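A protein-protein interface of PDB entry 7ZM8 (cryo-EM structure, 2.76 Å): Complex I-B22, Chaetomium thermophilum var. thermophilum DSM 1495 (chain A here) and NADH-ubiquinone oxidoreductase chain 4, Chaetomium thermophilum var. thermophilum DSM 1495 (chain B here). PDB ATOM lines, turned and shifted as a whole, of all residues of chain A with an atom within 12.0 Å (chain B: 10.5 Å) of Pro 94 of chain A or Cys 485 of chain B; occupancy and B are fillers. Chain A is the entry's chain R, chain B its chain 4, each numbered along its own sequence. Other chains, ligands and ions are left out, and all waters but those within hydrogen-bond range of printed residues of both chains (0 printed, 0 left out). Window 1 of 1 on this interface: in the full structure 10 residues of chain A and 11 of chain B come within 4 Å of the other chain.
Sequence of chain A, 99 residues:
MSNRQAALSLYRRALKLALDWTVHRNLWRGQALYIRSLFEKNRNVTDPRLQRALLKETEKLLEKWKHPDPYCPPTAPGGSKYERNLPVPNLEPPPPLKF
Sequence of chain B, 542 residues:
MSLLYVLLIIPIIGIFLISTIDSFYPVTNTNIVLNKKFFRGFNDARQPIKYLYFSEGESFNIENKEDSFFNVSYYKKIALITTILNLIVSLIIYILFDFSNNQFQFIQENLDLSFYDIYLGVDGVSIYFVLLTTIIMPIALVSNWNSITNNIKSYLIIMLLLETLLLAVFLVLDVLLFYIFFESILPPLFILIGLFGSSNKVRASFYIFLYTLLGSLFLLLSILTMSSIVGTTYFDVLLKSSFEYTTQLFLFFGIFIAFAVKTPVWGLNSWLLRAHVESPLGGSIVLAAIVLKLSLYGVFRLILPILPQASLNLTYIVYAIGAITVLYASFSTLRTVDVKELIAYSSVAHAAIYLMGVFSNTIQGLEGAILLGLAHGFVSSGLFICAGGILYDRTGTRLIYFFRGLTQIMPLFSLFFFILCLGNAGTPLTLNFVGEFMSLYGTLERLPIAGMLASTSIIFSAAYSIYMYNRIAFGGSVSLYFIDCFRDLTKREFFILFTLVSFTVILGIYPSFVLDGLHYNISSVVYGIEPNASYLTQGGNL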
ATOM      1  N   PRO A  87     -14.485  -3.526 -15.535  1.00  0.00           N
ATOM      2  CA  PRO A  87     -15.406  -4.387 -16.273  1.00  0.00           C
ATOM      3  C   PRO A  87     -15.450  -5.812 -15.720  1.00  0.00           C
ATOM      4  O   PRO A  87     -14.471  -6.211 -15.147  1.00  0.00           O
ATOM      5  CB  PRO A  87     -14.874  -4.283 -17.708  1.00  0.00           C
ATOM      6  CG  PRO A  87     -13.403  -4.013 -17.536  1.00  0.00           C
ATOM      7  CD  PRO A  87     -13.337  -3.101 -16.334  1.00  0.00           C
ATOM      8  N   VAL A  88     -16.563  -6.534 -15.883  1.00  0.00           N
ATOM      9  CA  VAL A  88     -16.555  -7.948 -15.499  1.00  0.00           C
ATOM     10  C   VAL A  88     -15.453  -8.662 -16.269  1.00  0.00           C
ATOM     11  O   VAL A  88     -15.340  -8.484 -17.497  1.00  0.00           O
ATOM     12  CB  VAL A  88     -17.928  -8.587 -15.775  1.00  0.00           C
ATOM     13  CG1 VAL A  88     -17.913 -10.057 -15.444  1.00  0.00           C
ATOM     14  CG2 VAL A  88     -19.010  -7.876 -14.984  1.00  0.00           C
ATOM     15  N   PRO A  89     -14.601  -9.453 -15.617  1.00  0.00           N
ATOM     16  CA  PRO A  89     -13.531 -10.154 -16.333  1.00  0.00           C
ATOM     17  C   PRO A  89     -13.986 -11.385 -17.099  1.00  0.00           C
ATOM     18  O   PRO A  89     -13.138 -12.172 -17.524  1.00  0.00           O
ATOM     19  CB  PRO A  89     -12.568 -10.555 -15.200  1.00  0.00           C
ATOM     20  CG  PRO A  89     -13.093  -9.908 -13.949  1.00  0.00           C
ATOM     21  CD  PRO A  89     -14.533  -9.679 -14.168  1.00  0.00           C
ATOM     22  N   ASN A  90     -15.292 -11.576 -17.273  1.00  0.00           N
ATOM     23  CA  ASN A  90     -15.832 -12.758 -17.936  1.00  0.00           C
ATOM     24  C   ASN A  90     -17.204 -12.368 -18.477  1.00  0.00           C
ATOM     25  O   ASN A  90     -18.186 -12.368 -17.731  1.00  0.00           O
ATOM     26  CB  ASN A  90     -15.923 -13.919 -16.956  1.00  0.00           C
ATOM     27  CG  ASN A  90     -16.216 -15.238 -17.626  1.00  0.00           C
ATOM     28  OD1 ASN A  90     -16.964 -15.309 -18.593  1.00  0.00           O
ATOM     29  ND2 ASN A  90     -15.642 -16.303 -17.088  1.00  0.00           N
ATOM     30  N   LEU A  91     -17.271 -12.049 -19.762  1.00  0.00           N
ATOM     31  CA  LEU A  91     -18.525 -11.623 -20.363  1.00  0.00           C
ATOM     32  C   LEU A  91     -19.279 -12.761 -21.031  1.00  0.00           C
ATOM     33  O   LEU A  91     -20.355 -12.530 -21.591  1.00  0.00           O
ATOM     34  CB  LEU A  91     -18.275 -10.508 -21.381  1.00  0.00           C
ATOM     35  CG  LEU A  91     -17.421  -9.316 -20.954  1.00  0.00           C
ATOM     36  CD1 LEU A  91     -17.418  -8.283 -22.056  1.00  0.00           C
ATOM     37  CD2 LEU A  91     -17.919  -8.717 -19.661  1.00  0.00           C
ATOM     38  N   GLU A  92     -18.753 -13.969 -20.994  1.00  0.00           N
ATOM     39  CA  GLU A  92     -19.447 -15.082 -21.614  1.00  0.00           C
ATOM     40  C   GLU A  92     -20.627 -15.525 -20.755  1.00  0.00           C
ATOM     41  O   GLU A  92     -20.569 -15.463 -19.524  1.00  0.00           O
ATOM     42  CB  GLU A  92     -18.496 -16.250 -21.824  1.00  0.00           C
ATOM     43  CG  GLU A  92     -17.393 -15.967 -22.825  1.00  0.00           C
ATOM     44  CD  GLU A  92     -17.920 -15.783 -24.235  1.00  0.00           C
ATOM     45  OE1 GLU A  92     -18.938 -16.417 -24.580  1.00  0.00           O
ATOM     46  OE2 GLU A  92     -17.316 -15.001 -24.998  1.00  0.00           O
ATOM     47  N   PRO A  93     -21.746 -15.914 -21.435  1.00  0.00           N
ATOM     48  CA  PRO A  93     -22.965 -16.296 -20.758  1.00  0.00           C
ATOM     49  C   PRO A  93     -22.632 -17.463 -19.831  1.00  0.00           C
ATOM     50  O   PRO A  93     -21.656 -18.139 -20.066  1.00  0.00           O
ATOM     51  CB  PRO A  93     -23.864 -16.720 -21.913  1.00  0.00           C
ATOM     52  CG  PRO A  93     -23.493 -15.791 -22.999  1.00  0.00           C
ATOM     53  CD  PRO A  93     -21.997 -15.917 -22.907  1.00  0.00           C
ATOM     54  N   PRO A  94     -23.416 -17.725 -18.769  1.00  0.00           N
ATOM     55  CA  PRO A  94     -23.061 -18.786 -17.852  1.00  0.00           C
ATOM     56  C   PRO A  94     -23.180 -20.137 -18.578  1.00  0.00           C
ATOM     57  O   PRO A  94     -23.990 -20.249 -19.462  1.00  0.00           O
ATOM     58  CB  PRO A  94     -24.056 -18.578 -16.700  1.00  0.00           C
ATOM     59  CG  PRO A  94     -24.610 -17.199 -16.903  1.00  0.00           C
ATOM     60  CD  PRO A  94     -24.645 -17.038 -18.405  1.00  0.00           C
ATOM     61  N   PRO A  95     -22.363 -21.159 -18.259  1.00  0.00           N
ATOM     62  CA  PRO A  95     -22.534 -22.484 -18.858  1.00  0.00           C
ATOM     63  C   PRO A  95     -23.895 -23.031 -18.408  1.00  0.00           C
ATOM     64  O   PRO A  95     -24.347 -22.658 -17.354  1.00  0.00           O
ATOM     65  CB  PRO A  95     -21.387 -23.328 -18.314  1.00  0.00           C
ATOM     66  CG  PRO A  95     -20.805 -22.521 -17.173  1.00  0.00           C
ATOM     67  CD  PRO A  95     -21.194 -21.076 -17.398  1.00  0.00           C
ATOM     68  N   PRO A  96     -24.564 -23.928 -19.158  1.00  0.00           N
ATOM     69  CA  PRO A  96     -25.941 -24.306 -18.816  1.00  0.00           C
ATOM     70  C   PRO A  96     -26.176 -25.328 -17.694  1.00  0.00           C
ATOM     71  O   PRO A  96     -26.477 -26.455 -17.993  1.00  0.00           O
ATOM     72  CB  PRO A  96     -26.423 -24.851 -20.162  1.00  0.00           C
ATOM     73  CG  PRO A  96     -25.196 -25.459 -20.802  1.00  0.00           C
ATOM     74  CD  PRO A  96     -24.049 -24.579 -20.359  1.00  0.00           C
ATOM     75  N   LEU A  97     -26.112 -24.889 -16.437  1.00  0.00           N
ATOM     76  CA  LEU A  97     -26.257 -25.802 -15.274  1.00  0.00           C
ATOM     77  C   LEU A  97     -27.495 -25.412 -14.452  1.00  0.00           C
ATOM     78  O   LEU A  97     -27.766 -24.213 -14.361  1.00  0.00           O
ATOM     79  CB  LEU A  97     -24.983 -25.754 -14.422  1.00  0.00           C
ATOM     80  CG  LEU A  97     -23.656 -26.041 -15.122  1.00  0.00           C
ATOM     81  CD1 LEU A  97     -22.554 -26.200 -14.092  1.00  0.00           C
ATOM     82  CD2 LEU A  97     -23.747 -27.282 -15.996  1.00  0.00           C
ATOM     83  N   LYS A  98     -28.189 -26.364 -13.821  1.00  0.00           N
ATOM     84  CA  LYS A  98     -29.463 -26.037 -13.122  1.00  0.00           C
ATOM     85  C   LYS A  98     -29.359 -26.202 -11.606  1.00  0.00           C
ATOM     86  O   LYS A  98     -28.914 -27.257 -11.150  1.00  0.00           O
ATOM     87  CB  LYS A  98     -30.531 -27.021 -13.608  1.00  0.00           C
ATOM     88  CG  LYS A  98     -31.140 -26.712 -14.969  1.00  0.00           C
ATOM     89  CD  LYS A  98     -32.017 -25.481 -14.957  1.00  0.00           C
ATOM     90  CE  LYS A  98     -33.177 -25.596 -13.989  1.00  0.00           C
ATOM     91  NZ  LYS A  98     -34.063 -26.734 -14.325  1.00  0.00           N
ATOM     92  N   PHE A  99     -29.792 -25.185 -10.860  1.00  0.00           N
ATOM     93  CA  PHE A  99     -29.609 -25.181  -9.383  1.00  0.00           C
ATOM     94  C   PHE A  99     -30.952 -25.140  -8.652  1.00  0.00           C
ATOM     95  O   PHE A  99     -30.974 -25.696  -7.528  1.00  0.00           O
ATOM     96  CB  PHE A  99     -28.716 -24.000  -8.981  1.00  0.00           C
ATOM     97  CG  PHE A  99     -27.311 -24.195  -9.477  1.00  0.00           C
ATOM     98  CD1 PHE A  99     -26.505 -25.177  -8.927  1.00  0.00           C
ATOM     99  CD2 PHE A  99     -26.820 -23.457 -10.539  1.00  0.00           C
ATOM    100  CE1 PHE A  99     -25.224 -25.386  -9.407  1.00  0.00           C
ATOM    101  CE2 PHE A  99     -25.540 -23.675 -11.016  1.00  0.00           C
ATOM    102  CZ  PHE A  99     -24.739 -24.630 -10.443  1.00  0.00           C
ATOM    103  N   ASP B 393     -24.032 -24.077  -3.643  1.00  0.00           N
ATOM    104  CA  ASP B 393     -24.617 -24.714  -4.845  1.00  0.00           C
ATOM    105  C   ASP B 393     -23.791 -24.401  -6.090  1.00  0.00           C
ATOM    106  O   ASP B 393     -23.609 -25.314  -6.891  1.00  0.00           O
ATOM    107  CB  ASP B 393     -26.087 -24.335  -5.037  1.00  0.00           C
ATOM    108  CG  ASP B 393     -27.039 -25.241  -4.280  1.00  0.00           C
ATOM    109  OD1 ASP B 393     -26.578 -25.925  -3.346  1.00  0.00           O
ATOM    110  OD2 ASP B 393     -28.230 -25.257  -4.634  1.00  0.00           O
ATOM    111  N   ARG B 394     -23.301 -23.179  -6.230  1.00  0.00           N
ATOM    112  CA  ARG B 394     -22.592 -22.778  -7.465  1.00  0.00           C
ATOM    113  C   ARG B 394     -21.087 -22.996  -7.393  1.00  0.00           C
ATOM    114  O   ARG B 394     -20.475 -23.065  -8.453  1.00  0.00           O
ATOM    115  CB  ARG B 394     -22.837 -21.294  -7.723  1.00  0.00           C
ATOM    116  CG  ARG B 394     -24.188 -20.982  -8.348  1.00  0.00           C
ATOM    117  CD  ARG B 394     -24.645 -19.586  -7.971  1.00  0.00           C
ATOM    118  NE  ARG B 394     -25.949 -19.251  -8.518  1.00  0.00           N
ATOM    119  CZ  ARG B 394     -27.103 -19.726  -8.068  1.00  0.00           C
ATOM    120  NH1 ARG B 394     -28.235 -19.352  -8.633  1.00  0.00           N
ATOM    121  NH2 ARG B 394     -27.123 -20.583  -7.066  1.00  0.00           N
ATOM    122  N   THR B 395     -20.507 -23.123  -6.209  1.00  0.00           N
ATOM    123  CA  THR B 395     -19.025 -23.158  -6.139  1.00  0.00           C
ATOM    124  C   THR B 395     -18.541 -24.445  -5.513  1.00  0.00           C
ATOM    125  O   THR B 395     -17.403 -24.809  -5.791  1.00  0.00           O
ATOM    126  CB  THR B 395     -18.510 -21.998  -5.281  1.00  0.00           C
ATOM    127  OG1 THR B 395     -19.001 -22.150  -3.951  1.00  0.00           O
ATOM    128  CG2 THR B 395     -18.929 -20.645  -5.801  1.00  0.00           C
ATOM    129  N   GLY B 405     -16.927  -9.431  -5.405  1.00  0.00           N
ATOM    130  CA  GLY B 405     -17.638  -8.735  -6.485  1.00  0.00           C
ATOM    131  C   GLY B 405     -18.831  -9.472  -7.013  1.00  0.00           C
ATOM    132  O   GLY B 405     -19.116  -9.306  -8.192  1.00  0.00           O
ATOM    133  N   LEU B 406     -19.528 -10.226  -6.173  1.00  0.00           N
ATOM    134  CA  LEU B 406     -20.618 -11.030  -6.701  1.00  0.00           C
ATOM    135  C   LEU B 406     -21.807 -10.197  -7.142  1.00  0.00           C
ATOM    136  O   LEU B 406     -22.644 -10.702  -7.894  1.00  0.00           O
ATOM    137  CB  LEU B 406     -21.073 -12.048  -5.663  1.00  0.00           C
ATOM    138  CG  LEU B 406     -20.358 -13.390  -5.709  1.00  0.00           C
ATOM    139  CD1 LEU B 406     -21.036 -14.338  -4.771  1.00  0.00           C
ATOM    140  CD2 LEU B 406     -20.358 -13.943  -7.120  1.00  0.00           C
ATOM    141  N   THR B 407     -21.846  -8.907  -6.808  1.00  0.00           N
ATOM    142  CA  THR B 407     -22.983  -8.018  -7.185  1.00  0.00           C
ATOM    143  C   THR B 407     -22.964  -7.762  -8.688  1.00  0.00           C
ATOM    144  O   THR B 407     -24.035  -7.572  -9.257  1.00  0.00           O
ATOM    145  CB  THR B 407     -22.958  -6.671  -6.453  1.00  0.00           C
ATOM    146  OG1 THR B 407     -24.033  -5.873  -6.942  1.00  0.00           O
ATOM    147  CG2 THR B 407     -21.679  -5.907  -6.673  1.00  0.00           C
ATOM    148  N   GLN B 408     -21.789  -7.773  -9.295  1.00  0.00           N
ATOM    149  CA  GLN B 408     -21.624  -7.465 -10.730  1.00  0.00           C
ATOM    150  C   GLN B 408     -22.378  -8.467 -11.605  1.00  0.00           C
ATOM    151  O   GLN B 408     -22.884  -8.059 -12.642  1.00  0.00           O
ATOM    152  CB  GLN B 408     -20.132  -7.375 -11.035  1.00  0.00           C
ATOM    153  CG  GLN B 408     -19.563  -5.970 -10.962  1.00  0.00           C
ATOM    154  CD  GLN B 408     -18.272  -5.836 -11.729  1.00  0.00           C
ATOM    155  OE1 GLN B 408     -17.402  -6.698 -11.677  1.00  0.00           O
ATOM    156  NE2 GLN B 408     -18.133  -4.736 -12.448  1.00  0.00           N
ATOM    157  N   ILE B 409     -22.423  -9.749 -11.238  1.00  0.00           N
ATOM    158  CA  ILE B 409     -23.025 -10.797 -12.117  1.00  0.00           C
ATOM    159  C   ILE B 409     -24.313 -11.324 -11.492  1.00  0.00           C
ATOM    160  O   ILE B 409     -25.093 -11.951 -12.201  1.00  0.00           O
ATOM    161  CB  ILE B 409     -22.005 -11.932 -12.355  1.00  0.00           C
ATOM    162  CG1 ILE B 409     -21.381 -12.426 -11.048  1.00  0.00           C
ATOM    163  CG2 ILE B 409     -20.951 -11.509 -13.365  1.00  0.00           C
ATOM    164  CD1 ILE B 409     -20.740 -13.782 -11.150  1.00  0.00           C
ATOM    165  N   MET B 410     -24.537 -11.033 -10.222  1.00  0.00           N
ATOM    166  CA  MET B 410     -25.720 -11.544  -9.495  1.00  0.00           C
ATOM    167  C   MET B 410     -26.349 -10.398  -8.713  1.00  0.00           C
ATOM    168  O   MET B 410     -26.277 -10.424  -7.495  1.00  0.00           O
ATOM    169  CB  MET B 410     -25.327 -12.662  -8.533  1.00  0.00           C
ATOM    170  CG  MET B 410     -24.711 -13.856  -9.216  1.00  0.00           C
ATOM    171  SD  MET B 410     -24.237 -15.104  -8.015  1.00  0.00           S
ATOM    172  CE  MET B 410     -25.840 -15.531  -7.341  1.00  0.00           C
ATOM    173  N   PRO B 411     -27.039  -9.457  -9.376  1.00  0.00           N
ATOM    174  CA  PRO B 411     -27.598  -8.285  -8.721  1.00  0.00           C
ATOM    175  C   PRO B 411     -28.847  -8.552  -7.880  1.00  0.00           C
ATOM    176  O   PRO B 411     -29.089  -7.790  -6.988  1.00  0.00           O
ATOM    177  CB  PRO B 411     -28.036  -7.431  -9.916  1.00  0.00           C
ATOM    178  CG  PRO B 411     -28.278  -8.389 -11.027  1.00  0.00           C
ATOM    179  CD  PRO B 411     -27.204  -9.423 -10.828  1.00  0.00           C
ATOM    180  N   VAL B 478     -15.640  -9.098  -9.896  1.00  0.00           N
ATOM    181  CA  VAL B 478     -15.926 -10.553  -9.797  1.00  0.00           C
ATOM    182  C   VAL B 478     -14.577 -11.262  -9.638  1.00  0.00           C
ATOM    183  O   VAL B 478     -13.646 -10.934 -10.383  1.00  0.00           O
ATOM    184  CB  VAL B 478     -16.754 -11.050 -11.004  1.00  0.00           C
ATOM    185  CG1 VAL B 478     -17.057 -12.535 -10.915  1.00  0.00           C
ATOM    186  CG2 VAL B 478     -18.031 -10.256 -11.192  1.00  0.00           C
ATOM    187  N   SER B 479     -14.511 -12.235  -8.723  1.00  0.00           N
ATOM    188  CA  SER B 479     -13.241 -12.932  -8.420  1.00  0.00           C
ATOM    189  C   SER B 479     -12.629 -13.524  -9.681  1.00  0.00           C
ATOM    190  O   SER B 479     -13.357 -13.736 -10.658  1.00  0.00           O
ATOM    191  CB  SER B 479     -13.505 -14.006  -7.422  1.00  0.00           C
ATOM    192  OG  SER B 479     -14.068 -15.141  -8.042  1.00  0.00           O
ATOM    193  N   LEU B 480     -11.353 -13.885  -9.615  1.00  0.00           N
ATOM    194  CA  LEU B 480     -10.686 -14.524 -10.765  1.00  0.00           C
ATOM    195  C   LEU B 480     -10.649 -16.028 -10.529  1.00  0.00           C
ATOM    196  O   LEU B 480     -10.235 -16.753 -11.438  1.00  0.00           O
ATOM    197  CB  LEU B 480      -9.287 -13.920 -10.923  1.00  0.00           C
ATOM    198  CG  LEU B 480      -9.236 -12.435 -11.259  1.00  0.00           C
ATOM    199  CD1 LEU B 480      -7.799 -12.006 -11.468  1.00  0.00           C
ATOM    200  CD2 LEU B 480     -10.060 -12.136 -12.499  1.00  0.00           C
ATOM    201  N   TYR B 481     -11.154 -16.474  -9.389  1.00  0.00           N
ATOM    202  CA  TYR B 481     -11.161 -17.920  -9.074  1.00  0.00           C
ATOM    203  C   TYR B 481     -12.364 -18.556  -9.763  1.00  0.00           C
ATOM    204  O   TYR B 481     -12.433 -19.775  -9.822  1.00  0.00           O
ATOM    205  CB  TYR B 481     -11.170 -18.134  -7.562  1.00  0.00           C
ATOM    206  CG  TYR B 481     -10.001 -17.576  -6.796  1.00  0.00           C
ATOM    207  CD1 TYR B 481      -8.785 -18.232  -6.766  1.00  0.00           C
ATOM    208  CD2 TYR B 481     -10.125 -16.409  -6.064  1.00  0.00           C
ATOM    209  CE1 TYR B 481      -7.711 -17.727  -6.055  1.00  0.00           C
ATOM    210  CE2 TYR B 481      -9.063 -15.891  -5.346  1.00  0.00           C
ATOM    211  CZ  TYR B 481      -7.850 -16.549  -5.347  1.00  0.00           C
ATOM    212  OH  TYR B 481      -6.803 -16.040  -4.640  1.00  0.00           O
ATOM    213  N   PHE B 482     -13.300 -17.745 -10.255  1.00  0.00           N
ATOM    214  CA  PHE B 482     -14.475 -18.199 -10.993  1.00  0.00           C
ATOM    215  C   PHE B 482     -14.071 -18.349 -12.451  1.00  0.00           C
ATOM    216  O   PHE B 482     -13.877 -17.361 -13.159  1.00  0.00           O
ATOM    217  CB  PHE B 482     -15.625 -17.213 -10.829  1.00  0.00           C
ATOM    218  CG  PHE B 482     -16.106 -17.062  -9.414  1.00  0.00           C
ATOM    219  CD1 PHE B 482     -15.717 -17.952  -8.430  1.00  0.00           C
ATOM    220  CD2 PHE B 482     -16.953 -16.026  -9.070  1.00  0.00           C
ATOM    221  CE1 PHE B 482     -16.162 -17.806  -7.126  1.00  0.00           C
ATOM    222  CE2 PHE B 482     -17.398 -15.878  -7.767  1.00  0.00           C
ATOM    223  CZ  PHE B 482     -17.004 -16.767  -6.795  1.00  0.00           C
ATOM    224  N   ILE B 483     -13.928 -19.594 -12.899  1.00  0.00           N
ATOM    225  CA  ILE B 483     -13.510 -19.852 -14.273  1.00  0.00           C
ATOM    226  C   ILE B 483     -14.626 -19.498 -15.246  1.00  0.00           C
ATOM    227  O   ILE B 483     -14.385 -18.916 -16.310  1.00  0.00           O
ATOM    228  CB  ILE B 483     -13.066 -21.316 -14.429  1.00  0.00           C
ATOM    229  CG1 ILE B 483     -11.831 -21.580 -13.577  1.00  0.00           C
ATOM    230  CG2 ILE B 483     -12.781 -21.636 -15.876  1.00  0.00           C
ATOM    231  CD1 ILE B 483     -11.401 -23.009 -13.579  1.00  0.00           C
ATOM    232  N   ASP B 484     -15.840 -19.922 -14.907  1.00  0.00           N
ATOM    233  CA  ASP B 484     -17.014 -19.634 -15.764  1.00  0.00           C
ATOM    234  C   ASP B 484     -17.992 -18.725 -15.014  1.00  0.00           C
ATOM    235  O   ASP B 484     -17.860 -18.621 -13.795  1.00  0.00           O
ATOM    236  CB  ASP B 484     -17.646 -20.945 -16.235  1.00  0.00           C
ATOM    237  CG  ASP B 484     -17.721 -22.011 -15.161  1.00  0.00           C
ATOM    238  OD1 ASP B 484     -17.777 -21.639 -13.981  1.00  0.00           O
ATOM    239  OD2 ASP B 484     -17.720 -23.199 -15.521  1.00  0.00           O
ATOM    240  N   CYS B 485     -18.896 -18.060 -15.727  1.00  0.00           N
ATOM    241  CA  CYS B 485     -19.882 -17.150 -15.088  1.00  0.00           C
ATOM    242  C   CYS B 485     -20.925 -17.924 -14.282  1.00  0.00           C
ATOM    243  O   CYS B 485     -21.299 -19.025 -14.694  1.00  0.00           O
ATOM    244  CB  CYS B 485     -20.579 -16.245 -16.091  1.00  0.00           C
ATOM    245  SG  CYS B 485     -21.416 -14.845 -15.308  1.00  0.00           S
ATOM    246  N   PHE B 486     -21.412 -17.324 -13.201  1.00  0.00           N
ATOM    247  CA  PHE B 486     -22.448 -17.968 -12.367  1.00  0.00           C
ATOM    248  C   PHE B 486     -23.788 -17.358 -12.724  1.00  0.00           C
ATOM    249  O   PHE B 486     -23.844 -16.141 -12.884  1.00  0.00           O
ATOM    250  CB  PHE B 486     -22.267 -17.599 -10.901  1.00  0.00           C
ATOM    251  CG  PHE B 486     -21.069 -18.218 -10.239  1.00  0.00           C
ATOM    252  CD1 PHE B 486     -20.258 -19.102 -10.929  1.00  0.00           C
ATOM    253  CD2 PHE B 486     -20.762 -17.917  -8.927  1.00  0.00           C
ATOM    254  CE1 PHE B 486     -19.153 -19.668 -10.321  1.00  0.00           C
ATOM    255  CE2 PHE B 486     -19.665 -18.493  -8.318  1.00  0.00           C
ATOM    256  CZ  PHE B 486     -18.864 -19.362  -9.016  1.00  0.00           C
ATOM    257  N   ARG B 487     -24.836 -18.174 -12.801  1.00  0.00           N
ATOM    258  CA  ARG B 487     -26.189 -17.619 -13.036  1.00  0.00           C
ATOM    259  C   ARG B 487     -26.633 -16.873 -11.773  1.00  0.00           C
ATOM    260  O   ARG B 487     -26.098 -17.162 -10.691  1.00  0.00           O
ATOM    261  CB  ARG B 487     -27.169 -18.739 -13.396  1.00  0.00           C
ATOM    262  CG  ARG B 487     -27.464 -19.707 -12.261  1.00  0.00           C
ATOM    263  CD  ARG B 487     -28.349 -20.842 -12.725  1.00  0.00           C
ATOM    264  NE  ARG B 487     -29.536 -20.386 -13.431  1.00  0.00           N
ATOM    265  CZ  ARG B 487     -30.467 -21.198 -13.911  1.00  0.00           C
ATOM    266  NH1 ARG B 487     -31.518 -20.706 -14.543  1.00  0.00           N
ATOM    267  NH2 ARG B 487     -30.347 -22.503 -13.752  1.00  0.00           N
ATOM    268  N   ASP B 488     -27.597 -15.965 -11.911  1.00  0.00           N
ATOM    269  CA  ASP B 488     -28.141 -15.224 -10.749  1.00  0.00           C
ATOM    270  C   ASP B 488     -29.251 -16.062 -10.110  1.00  0.00           C
ATOM    271  O   ASP B 488     -29.347 -17.254 -10.430  1.00  0.00           O
ATOM    272  CB  ASP B 488     -28.566 -13.813 -11.163  1.00  0.00           C
ATOM    273  CG  ASP B 488     -28.902 -12.853 -10.035  1.00  0.00           C
ATOM    274  OD1 ASP B 488     -28.611 -13.175  -8.869  1.00  0.00           O
ATOM    275  OD2 ASP B 488     -29.459 -11.787 -10.337  1.00  0.00           O
ATOM    276  N   LEU B 489     -30.025 -15.464  -9.208  1.00  0.00           N
ATOM    277  CA  LEU B 489     -31.082 -16.176  -8.458  1.00  0.00           C
ATOM    278  C   LEU B 489     -32.075 -16.877  -9.378  1.00  0.00           C
ATOM    279  O   LEU B 489     -32.429 -16.303 -10.415  1.00  0.00           O
ATOM    280  CB  LEU B 489     -31.799 -15.147  -7.581  1.00  0.00           C
ATOM    281  CG  LEU B 489     -31.081 -14.765  -6.290  1.00  0.00           C
ATOM    282  CD1 LEU B 489     -32.051 -14.117  -5.317  1.00  0.00           C
ATOM    283  CD2 LEU B 489     -30.432 -15.984  -5.657  1.00  0.00           C
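The side-chain amide nitrogen (ND2) of Asn 90 of chain A lies within hydrogen-bond range of the backbone carbonyl oxygen (O) of Ile 483 of chain B (3.0 Å). The guanidinium group of Arg 487 of chain B is in hydrogen-bond range of the backbone carbonyl oxygen of Leu 97 of chain A (3.2 Å).
The side-chain amide oxygen of Asn 90 of chain A sits at hydrogen-bond distance from the backbone NH of Glu 92 of chain A (3.3 Å). O of Arg 487 of chain B lies within hydrogen-bond range of NE of Arg 394 of chain B (3.0 Å). N of Val 478 of chain B is in hydrogen-bond range of OE1 of Gln 408 of chain B (3.5 Å).
Val 88 of chain A touches Gln 408 of chain B (CG2 to OE1, 3.9 Å). CG of Pro 89 of chain A touches O of Val 478 of chain B (3.8 Å). Asn 90 of chain A touches Cys 485 of chain B. Glu 92 of chain A touches Cys 485 of chain B (O to CB, 3.5 Å). Pro 94 of chain A touches Cys 485 of chain B. Pro 94 of chain A touches Arg 487 of chain B. CG of Pro 95 of chain A touches OD2 of Asp 484 of chain B, 3.6 Å away. O of Cys 485 of chain B touches CD of Pro 95 of chain A (3.4 Å). Lys 98 of chain A touches Arg 487 of chain B (CD to NH2, 3.6 Å). Phe 99 of chain A touches Asp 393 of chain B.
Of chain A, only Asn 90 (3.9 Å), Glu 92 (3.5 Å), Pro 94 (3.4 Å) and Pro 95 (3.4 Å) come within 4 Å of Cys 485 of chain B. No residue of chain B comes within 4 Å of Pro 93 of chain A. Pro 95 of chain A touches two residues of chain B. Of chain A, only Val 88 (3.96 Å) comes within 4 Å of Ile 409 of chain B. Of the printed residues of chain B, Phe 99 of chain A touches Asp 393 and Arg 487. Of the printed residues of chain B, Lys 98 of chain A touches Arg 487. Printed residues of chain B within 4 Å of Asn 90 of chain A: Ile 483, Asp 484 and Cys 485. Of the printed residues of chain A, Val 478 of chain B touches Pro 89 (3.8 Å). Printed residues of chain B within 4 Å of Val 88 of chain A: Gln 408 and Ile 409. Leu 406 of chain B touches none of the printed residues of chain A. The nearest printed residue of chain B that does not touch Pro 94 of chain A is Phe 486 of chain B (4.2 Å).
Of the 22 printed residues of chain B, 8 touch a printed residue of chain A. Printed residues of chain B that touch a printed residue of chain A: Asp 393, Gln 408, Ile 409, Val 478, Ile 483, Asp 484, Cys 485 and Arg 487. Hydrophobic or aromatic side chains of chain B within 4 Å of the printed part of chain A: Ile 409. Of the 13 printed residues of chain A, 9 touch a printed residue of chain B. Hydrophobic or aromatic side chains of chain A that line the printed part of chain B: Val 88, Pro 89, Pro 94, Pro 95 and Phe 99. Among the printed residues, 15 pairs touch across the chains.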
